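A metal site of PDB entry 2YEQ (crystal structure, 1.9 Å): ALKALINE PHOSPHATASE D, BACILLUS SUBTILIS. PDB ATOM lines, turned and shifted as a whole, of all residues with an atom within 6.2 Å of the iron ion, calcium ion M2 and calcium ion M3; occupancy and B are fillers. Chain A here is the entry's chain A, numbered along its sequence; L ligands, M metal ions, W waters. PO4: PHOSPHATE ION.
The iron ion is bound by OH of Tyr 154, OD2 of Asp 151, NE2 of His 382, O3 of the ligand, O4 of the ligand and SG of Cys 124.
Within 4 Å of calcium ion M2: Asp 151, Asp 209, Asp 210 and Asp 380.
Calcium ion M3 is bound by water W1, OD2 of Asp 210, OD1 of Asn 215, OD1 of Asn 216, water W2 and O2 of the ligand.
Calcium ion M3 has six donor atoms within binding distance.
Water W2 lies within hydrogen-bond range of OD2 of Asp 350 (2.8 Å) and NH2 of Arg 279 (3.5 Å).
N of Asp 380 lies close to SG of Cys 124, at 3.8 Å.
The guanidinium group (NH2) of Arg 279 sits close to the side-chain carboxylate (OD1) of Asp 210, at 3.9 Å.
N of Cys 124 is in hydrogen-bond range of O of Gly 150 (2.9 Å).
A ring nitrogen (NE2) of His 211 sits at hydrogen-bond distance from a ring nitrogen (NE2) of His 510 (3.1 Å).
The side-chain hydroxyl (OG) of Ser 412 lies within hydrogen-bond range of the backbone carbonyl oxygen (O) of Cys 124, 3.1 Å away.
The backbone carbonyl oxygen of Asp 151 sits at hydrogen-bond distance from the backbone NH of Gln 125, 3.2 Å away.
The side-chain carboxylate (OD1) of Asp 151 is in hydrogen-bond range of the backbone NH (N) of His 211 (3.1 Å).
OH of Tyr 154 sits close to OG of Ser 412 (2.6 Å).
Calcium ion M2 is bound by the side-chain carboxylate (OD2) of Asp 209, 2.3 Å away.
Calcium ion M2 is bound by O2 of the ligand (2.3 Å).
The side-chain carboxylate (OD1) of Asp 380 binds calcium ion M2 (2.4 Å).
OD1 of Asp 210 binds calcium ion M2 (2.4 Å).
Calcium ion M2 is bound by OD2 of Asp 151 (2.5 Å).
Calcium ion M2 is bound by water W3 (2.6 Å).
Calcium ion M2 is bound by O4 of the ligand.
Slightly farther from calcium ion M2 lies OD1 of Asp 151 (2.9 Å).
His 211 touches calcium ion M3 (NE2 to CA, 3.7 Å).
Within 4 Å of calcium ion M3: Asp 210, His 211, Asn 215 and Asn 216.
Along chain A the residues within 4 Å of calcium ion M3 span positions 210 to 216.
The nearest printed residue that does not touch calcium ion M3 is His 510 (4.3 Å).
Within 4 Å of the iron ion: Cys 124, Asp 151, Tyr 154 and His 382.
The nearest printed residue that does not touch the iron ion is Ser 412 (4.03 Å).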
ATOM      1  N   SER A 123      19.840  20.461  -4.916  1.00  0.00           N
ATOM      2  CA  SER A 123      19.112  21.677  -4.514  1.00  0.00           C
ATOM      3  C   SER A 123      18.013  21.931  -5.506  1.00  0.00           C
ATOM      4  O   SER A 123      18.000  21.356  -6.594  1.00  0.00           O
ATOM      5  CB  SER A 123      20.085  22.859  -4.492  1.00  0.00           C
ATOM      6  OG  SER A 123      20.516  23.162  -5.798  1.00  0.00           O
ATOM      7  N   CYS A 124      17.089  22.835  -5.144  1.00  0.00           N
ATOM      8  CA  CYS A 124      16.223  23.505  -6.121  1.00  0.00           C
ATOM      9  C   CYS A 124      15.265  22.578  -6.898  1.00  0.00           C
ATOM     10  O   CYS A 124      15.443  22.246  -8.092  1.00  0.00           O
ATOM     11  CB  CYS A 124      17.032  24.428  -7.049  1.00  0.00           C
ATOM     12  SG  CYS A 124      17.876  25.837  -6.173  1.00  0.00           S
ATOM     13  N   GLN A 125      14.185  22.233  -6.210  1.00  0.00           N
ATOM     14  CA  GLN A 125      13.236  21.253  -6.722  1.00  0.00           C
ATOM     15  C   GLN A 125      11.814  21.798  -6.892  1.00  0.00           C
ATOM     16  O   GLN A 125      10.859  21.171  -6.439  1.00  0.00           O
ATOM     17  CB  GLN A 125      13.251  20.008  -5.830  1.00  0.00           C
ATOM     18  CG  GLN A 125      12.986  20.233  -4.357  1.00  0.00           C
ATOM     19  CD  GLN A 125      13.533  19.147  -3.509  1.00  0.00           C
ATOM     20  OE1 GLN A 125      14.607  18.587  -3.807  1.00  0.00           O
ATOM     21  NE2 GLN A 125      12.847  18.839  -2.406  1.00  0.00           N
ATOM     22  N   GLY A 150      19.381  23.521  -0.401  1.00  0.00           N
ATOM     23  CA  GLY A 150      18.297  24.546  -0.286  1.00  0.00           C
ATOM     24  C   GLY A 150      17.266  24.512  -1.396  1.00  0.00           C
ATOM     25  O   GLY A 150      17.411  23.793  -2.380  1.00  0.00           O
ATOM     26  N   ASP A 151      16.238  25.360  -1.221  1.00  0.00           N
ATOM     27  CA  ASP A 151      15.077  25.402  -2.064  1.00  0.00           C
ATOM     28  C   ASP A 151      14.490  23.994  -2.158  1.00  0.00           C
ATOM     29  O   ASP A 151      14.138  23.531  -3.239  1.00  0.00           O
ATOM     30  CB  ASP A 151      15.370  26.007  -3.427  1.00  0.00           C
ATOM     31  CG  ASP A 151      15.744  27.491  -3.370  1.00  0.00           C
ATOM     32  OD1 ASP A 151      15.835  28.062  -2.270  1.00  0.00           O
ATOM     33  OD2 ASP A 151      15.992  28.065  -4.471  1.00  0.00           O
ATOM     34  N   TYR A 154       9.335  25.553  -2.554  1.00  0.00           N
ATOM     35  CA  TYR A 154       9.146  26.924  -3.001  1.00  0.00           C
ATOM     36  C   TYR A 154       7.794  27.383  -2.419  1.00  0.00           C
ATOM     37  O   TYR A 154       6.914  26.549  -2.153  1.00  0.00           O
ATOM     38  CB  TYR A 154       9.159  27.069  -4.536  1.00  0.00           C
ATOM     39  CG  TYR A 154      10.543  26.909  -5.137  1.00  0.00           C
ATOM     40  CD1 TYR A 154      11.205  25.672  -5.118  1.00  0.00           C
ATOM     41  CD2 TYR A 154      11.217  27.993  -5.679  1.00  0.00           C
ATOM     42  CE1 TYR A 154      12.483  25.518  -5.631  1.00  0.00           C
ATOM     43  CE2 TYR A 154      12.512  27.864  -6.213  1.00  0.00           C
ATOM     44  CZ  TYR A 154      13.138  26.626  -6.172  1.00  0.00           C
ATOM     45  OH  TYR A 154      14.388  26.466  -6.701  1.00  0.00           O
ATOM     46  N   TYR A 161       5.632  31.577 -10.472  1.00  0.00           N
ATOM     47  CA  TYR A 161       7.011  31.359 -10.890  1.00  0.00           C
ATOM     48  C   TYR A 161       6.999  30.292 -11.975  1.00  0.00           C
ATOM     49  O   TYR A 161       6.976  29.096 -11.684  1.00  0.00           O
ATOM     50  CB  TYR A 161       7.840  30.919  -9.699  1.00  0.00           C
ATOM     51  CG  TYR A 161       9.287  30.576 -10.020  1.00  0.00           C
ATOM     52  CD1 TYR A 161       9.967  31.153 -11.090  1.00  0.00           C
ATOM     53  CD2 TYR A 161       9.961  29.656  -9.241  1.00  0.00           C
ATOM     54  CE1 TYR A 161      11.266  30.824 -11.366  1.00  0.00           C
ATOM     55  CE2 TYR A 161      11.275  29.334  -9.501  1.00  0.00           C
ATOM     56  CZ  TYR A 161      11.920  29.916 -10.559  1.00  0.00           C
ATOM     57  OH  TYR A 161      13.217  29.552 -10.829  1.00  0.00           O
ATOM     58  N   ASP A 209      17.978  27.231   1.840  1.00  0.00           N
ATOM     59  CA  ASP A 209      18.321  28.508   1.235  1.00  0.00           C
ATOM     60  C   ASP A 209      17.093  29.431   1.404  1.00  0.00           C
ATOM     61  O   ASP A 209      16.488  29.411   2.486  1.00  0.00           O
ATOM     62  CB  ASP A 209      18.764  28.379  -0.238  1.00  0.00           C
ATOM     63  CG  ASP A 209      19.406  29.673  -0.767  1.00  0.00           C
ATOM     64  OD1 ASP A 209      20.125  30.373   0.011  1.00  0.00           O
ATOM     65  OD2 ASP A 209      19.138  30.027  -1.976  1.00  0.00           O
ATOM     66  N   ASP A 210      16.710  30.183   0.387  1.00  0.00           N
ATOM     67  CA  ASP A 210      15.670  31.223   0.589  1.00  0.00           C
ATOM     68  C   ASP A 210      14.250  30.712   0.489  1.00  0.00           C
ATOM     69  O   ASP A 210      13.398  31.131   1.274  1.00  0.00           O
ATOM     70  CB  ASP A 210      15.830  32.448  -0.340  1.00  0.00           C
ATOM     71  CG  ASP A 210      16.035  32.097  -1.788  1.00  0.00           C
ATOM     72  OD1 ASP A 210      16.499  30.953  -2.099  1.00  0.00           O
ATOM     73  OD2 ASP A 210      15.768  32.963  -2.655  1.00  0.00           O
ATOM     74  N   HIS A 211      13.996  29.804  -0.461  1.00  0.00           N
ATOM     75  CA  HIS A 211      12.636  29.418  -0.775  1.00  0.00           C
ATOM     76  C   HIS A 211      11.943  28.535   0.244  1.00  0.00           C
ATOM     77  O   HIS A 211      10.723  28.374   0.169  1.00  0.00           O
ATOM     78  CB  HIS A 211      12.546  28.854  -2.174  1.00  0.00           C
ATOM     79  CG  HIS A 211      12.634  29.891  -3.254  1.00  0.00           C
ATOM     80  ND1 HIS A 211      11.618  30.795  -3.498  1.00  0.00           N
ATOM     81  CD2 HIS A 211      13.575  30.108  -4.201  1.00  0.00           C
ATOM     82  CE1 HIS A 211      11.942  31.526  -4.563  1.00  0.00           C
ATOM     83  NE2 HIS A 211      13.131  31.147  -4.990  1.00  0.00           N
ATOM     84  N   ASN A 215      11.468  33.973  -1.344  1.00  0.00           N
ATOM     85  CA  ASN A 215      12.534  34.408  -2.256  1.00  0.00           C
ATOM     86  C   ASN A 215      13.406  35.572  -1.734  1.00  0.00           C
ATOM     87  O   ASN A 215      12.880  36.647  -1.371  1.00  0.00           O
ATOM     88  CB  ASN A 215      11.961  34.842  -3.606  1.00  0.00           C
ATOM     89  CG  ASN A 215      13.048  35.030  -4.662  1.00  0.00           C
ATOM     90  OD1 ASN A 215      13.850  34.107  -4.916  1.00  0.00           O
ATOM     91  ND2 ASN A 215      13.070  36.207  -5.296  1.00  0.00           N
ATOM     92  N   ASN A 216      14.720  35.341  -1.749  1.00  0.00           N
ATOM     93  CA  ASN A 216      15.749  36.346  -1.477  1.00  0.00           C
ATOM     94  C   ASN A 216      15.619  37.074  -0.163  1.00  0.00           C
ATOM     95  O   ASN A 216      16.031  38.248  -0.046  1.00  0.00           O
ATOM     96  CB  ASN A 216      15.849  37.353  -2.627  1.00  0.00           C
ATOM     97  CG  ASN A 216      16.603  36.784  -3.858  1.00  0.00           C
ATOM     98  OD1 ASN A 216      16.441  35.626  -4.192  1.00  0.00           O
ATOM     99  ND2 ASN A 216      17.404  37.614  -4.532  1.00  0.00           N
ATOM    100  N   ARG A 279      21.569  32.345   5.006  1.00  0.00           N
ATOM    101  CA  ARG A 279      20.329  33.122   4.992  1.00  0.00           C
ATOM    102  C   ARG A 279      19.962  33.733   6.327  1.00  0.00           C
ATOM    103  O   ARG A 279      19.528  34.889   6.354  1.00  0.00           O
ATOM    104  CB  ARG A 279      19.121  32.261   4.572  1.00  0.00           C
ATOM    105  CG  ARG A 279      19.049  31.998   3.122  1.00  0.00           C
ATOM    106  CD  ARG A 279      18.773  33.179   2.276  1.00  0.00           C
ATOM    107  NE  ARG A 279      19.051  32.859   0.880  1.00  0.00           N
ATOM    108  CZ  ARG A 279      19.182  33.724  -0.116  1.00  0.00           C
ATOM    109  NH1 ARG A 279      19.011  35.057   0.066  1.00  0.00           N
ATOM    110  NH2 ARG A 279      19.491  33.274  -1.319  1.00  0.00           N
ATOM    111  N   GLN A 331      25.051  27.367   0.185  1.00  0.00           N
ATOM    112  CA  GLN A 331      23.904  27.646  -0.675  1.00  0.00           C
ATOM    113  C   GLN A 331      24.185  28.282  -2.001  1.00  0.00           C
ATOM    114  O   GLN A 331      23.519  27.964  -3.000  1.00  0.00           O
ATOM    115  CB  GLN A 331      22.932  28.574   0.077  1.00  0.00           C
ATOM    116  CG  GLN A 331      22.271  27.973   1.304  1.00  0.00           C
ATOM    117  CD  GLN A 331      23.177  27.791   2.502  1.00  0.00           C
ATOM    118  OE1 GLN A 331      24.194  28.483   2.674  1.00  0.00           O
ATOM    119  NE2 GLN A 331      22.793  26.854   3.385  1.00  0.00           N
ATOM    120  N   ILE A 332      25.105  29.253  -2.007  1.00  0.00           N
ATOM    121  CA  ILE A 332      25.159  30.223  -3.077  1.00  0.00           C
ATOM    122  C   ILE A 332      26.558  30.327  -3.748  1.00  0.00           C
ATOM    123  O   ILE A 332      27.574  29.923  -3.202  1.00  0.00           O
ATOM    124  CB  ILE A 332      24.724  31.632  -2.556  1.00  0.00           C
ATOM    125  CG1 ILE A 332      25.426  31.960  -1.249  1.00  0.00           C
ATOM    126  CG2 ILE A 332      23.156  31.711  -2.383  1.00  0.00           C
ATOM    127  CD1 ILE A 332      25.411  33.457  -0.879  1.00  0.00           C
ATOM    128  N   ASP A 350      23.035  38.650  -4.565  1.00  0.00           N
ATOM    129  CA  ASP A 350      22.563  37.606  -3.627  1.00  0.00           C
ATOM    130  C   ASP A 350      23.567  36.474  -3.384  1.00  0.00           C
ATOM    131  O   ASP A 350      23.398  35.657  -2.478  1.00  0.00           O
ATOM    132  CB  ASP A 350      21.244  37.037  -4.153  1.00  0.00           C
ATOM    133  CG  ASP A 350      20.532  36.174  -3.124  1.00  0.00           C
ATOM    134  OD1 ASP A 350      20.266  36.634  -1.982  1.00  0.00           O
ATOM    135  OD2 ASP A 350      20.220  35.005  -3.491  1.00  0.00           O
ATOM    136  N   ASP A 380      21.461  26.863  -5.773  1.00  0.00           N
ATOM    137  CA  ASP A 380      20.829  28.195  -6.001  1.00  0.00           C
ATOM    138  C   ASP A 380      20.675  28.644  -7.437  1.00  0.00           C
ATOM    139  O   ASP A 380      19.630  29.198  -7.799  1.00  0.00           O
ATOM    140  CB  ASP A 380      21.475  29.296  -5.140  1.00  0.00           C
ATOM    141  CG  ASP A 380      20.731  30.647  -5.263  1.00  0.00           C
ATOM    142  OD1 ASP A 380      19.563  30.763  -4.787  1.00  0.00           O
ATOM    143  OD2 ASP A 380      21.327  31.566  -5.890  1.00  0.00           O
ATOM    144  N   VAL A 381      21.674  28.371  -8.267  1.00  0.00           N
ATOM    145  CA  VAL A 381      21.742  29.002  -9.582  1.00  0.00           C
ATOM    146  C   VAL A 381      21.136  28.207 -10.714  1.00  0.00           C
ATOM    147  O   VAL A 381      21.083  28.668 -11.839  1.00  0.00           O
ATOM    148  CB  VAL A 381      23.216  29.479  -9.932  1.00  0.00           C
ATOM    149  CG1 VAL A 381      23.772  30.343  -8.768  1.00  0.00           C
ATOM    150  CG2 VAL A 381      24.137  28.291 -10.279  1.00  0.00           C
ATOM    151  N   HIS A 382      20.603  27.028 -10.403  1.00  0.00           N
ATOM    152  CA  HIS A 382      19.792  26.249 -11.357  1.00  0.00           C
ATOM    153  C   HIS A 382      20.581  25.843 -12.618  1.00  0.00           C
ATOM    154  O   HIS A 382      20.048  25.747 -13.704  1.00  0.00           O
ATOM    155  CB  HIS A 382      18.507  26.999 -11.755  1.00  0.00           C
ATOM    156  CG  HIS A 382      17.608  27.359 -10.589  1.00  0.00           C
ATOM    157  ND1 HIS A 382      16.498  28.158 -10.766  1.00  0.00           N
ATOM    158  CD2 HIS A 382      17.645  27.045  -9.280  1.00  0.00           C
ATOM    159  CE1 HIS A 382      15.887  28.328  -9.602  1.00  0.00           C
ATOM    160  NE2 HIS A 382      16.555  27.667  -8.673  1.00  0.00           N
ATOM    161  N   SER A 409      19.915  22.342 -10.625  1.00  0.00           N
ATOM    162  CA  SER A 409      18.688  22.106  -9.877  1.00  0.00           C
ATOM    163  C   SER A 409      18.082  20.729 -10.237  1.00  0.00           C
ATOM    164  O   SER A 409      18.268  20.238 -11.353  1.00  0.00           O
ATOM    165  CB  SER A 409      17.715  23.185 -10.256  1.00  0.00           C
ATOM    166  OG  SER A 409      17.644  23.351 -11.662  1.00  0.00           O
ATOM    167  N   SER A 412      14.124  23.093 -10.910  1.00  0.00           N
ATOM    168  CA  SER A 412      13.827  24.532 -11.094  1.00  0.00           C
ATOM    169  C   SER A 412      14.407  25.005 -12.398  1.00  0.00           C
ATOM    170  O   SER A 412      15.577  24.741 -12.703  1.00  0.00           O
ATOM    171  CB  SER A 412      14.395  25.369  -9.943  1.00  0.00           C
ATOM    172  OG  SER A 412      13.948  24.867  -8.714  1.00  0.00           O
ATOM    173  N   ARG A 506      16.594  34.144 -14.603  1.00  0.00           N
ATOM    174  CA  ARG A 506      16.219  33.656 -13.286  1.00  0.00           C
ATOM    175  C   ARG A 506      15.678  34.810 -12.393  1.00  0.00           C
ATOM    176  O   ARG A 506      14.617  34.683 -11.798  1.00  0.00           O
ATOM    177  CB  ARG A 506      17.391  32.915 -12.632  1.00  0.00           C
ATOM    178  CG  ARG A 506      17.071  32.242 -11.304  1.00  0.00           C
ATOM    179  CD  ARG A 506      18.162  31.296 -10.877  1.00  0.00           C
ATOM    180  NE  ARG A 506      19.460  31.969 -10.780  1.00  0.00           N
ATOM    181  CZ  ARG A 506      20.037  32.408  -9.658  1.00  0.00           C
ATOM    182  NH1 ARG A 506      19.476  32.246  -8.455  1.00  0.00           N
ATOM    183  NH2 ARG A 506      21.230  33.008  -9.746  1.00  0.00           N
ATOM    184  N   HIS A 510      11.632  35.299 -11.318  1.00  0.00           N
ATOM    185  CA  HIS A 510      11.210  35.517  -9.933  1.00  0.00           C
ATOM    186  C   HIS A 510      10.488  36.876  -9.739  1.00  0.00           C
ATOM    187  O   HIS A 510       9.602  36.973  -8.892  1.00  0.00           O
ATOM    188  CB  HIS A 510      12.403  35.452  -9.000  1.00  0.00           C
ATOM    189  CG  HIS A 510      12.904  34.071  -8.746  1.00  0.00           C
ATOM    190  ND1 HIS A 510      13.734  33.399  -9.623  1.00  0.00           N
ATOM    191  CD2 HIS A 510      12.712  33.230  -7.707  1.00  0.00           C
ATOM    192  CE1 HIS A 510      14.038  32.219  -9.132  1.00  0.00           C
ATOM    193  NE2 HIS A 510      13.438  32.091  -7.960  1.00  0.00           N
HETATM  194  P   PO4 L   1      16.441  30.434  -6.620  1.00  0.00           P
HETATM  195  O1  PO4 L   1      16.892  31.314  -7.718  1.00  0.00           O
HETATM  196  O2  PO4 L   1      16.448  31.014  -5.240  1.00  0.00           O
HETATM  197  O3  PO4 L   1      15.197  29.648  -6.994  1.00  0.00           O
HETATM  198  O4  PO4 L   1      17.535  29.350  -6.362  1.00  0.00           O
HETATM  199 FE    FE M   1      16.068  27.537  -6.559  1.00  0.00          FE
HETATM  200 CA    CA M   2      17.697  29.764  -3.751  1.00  0.00          CA
HETATM  201 CA    CA M   3      16.096  33.395  -4.872  1.00  0.00          CA
HETATM  202  O   HOH W   1      16.282  33.822  -7.053  1.00  0.00           O
HETATM  203  O   HOH W   2      18.438  33.226  -4.611  1.00  0.00           O
HETATM  204  O   HOH W   3      18.755  27.422  -3.568  1.00  0.00           O
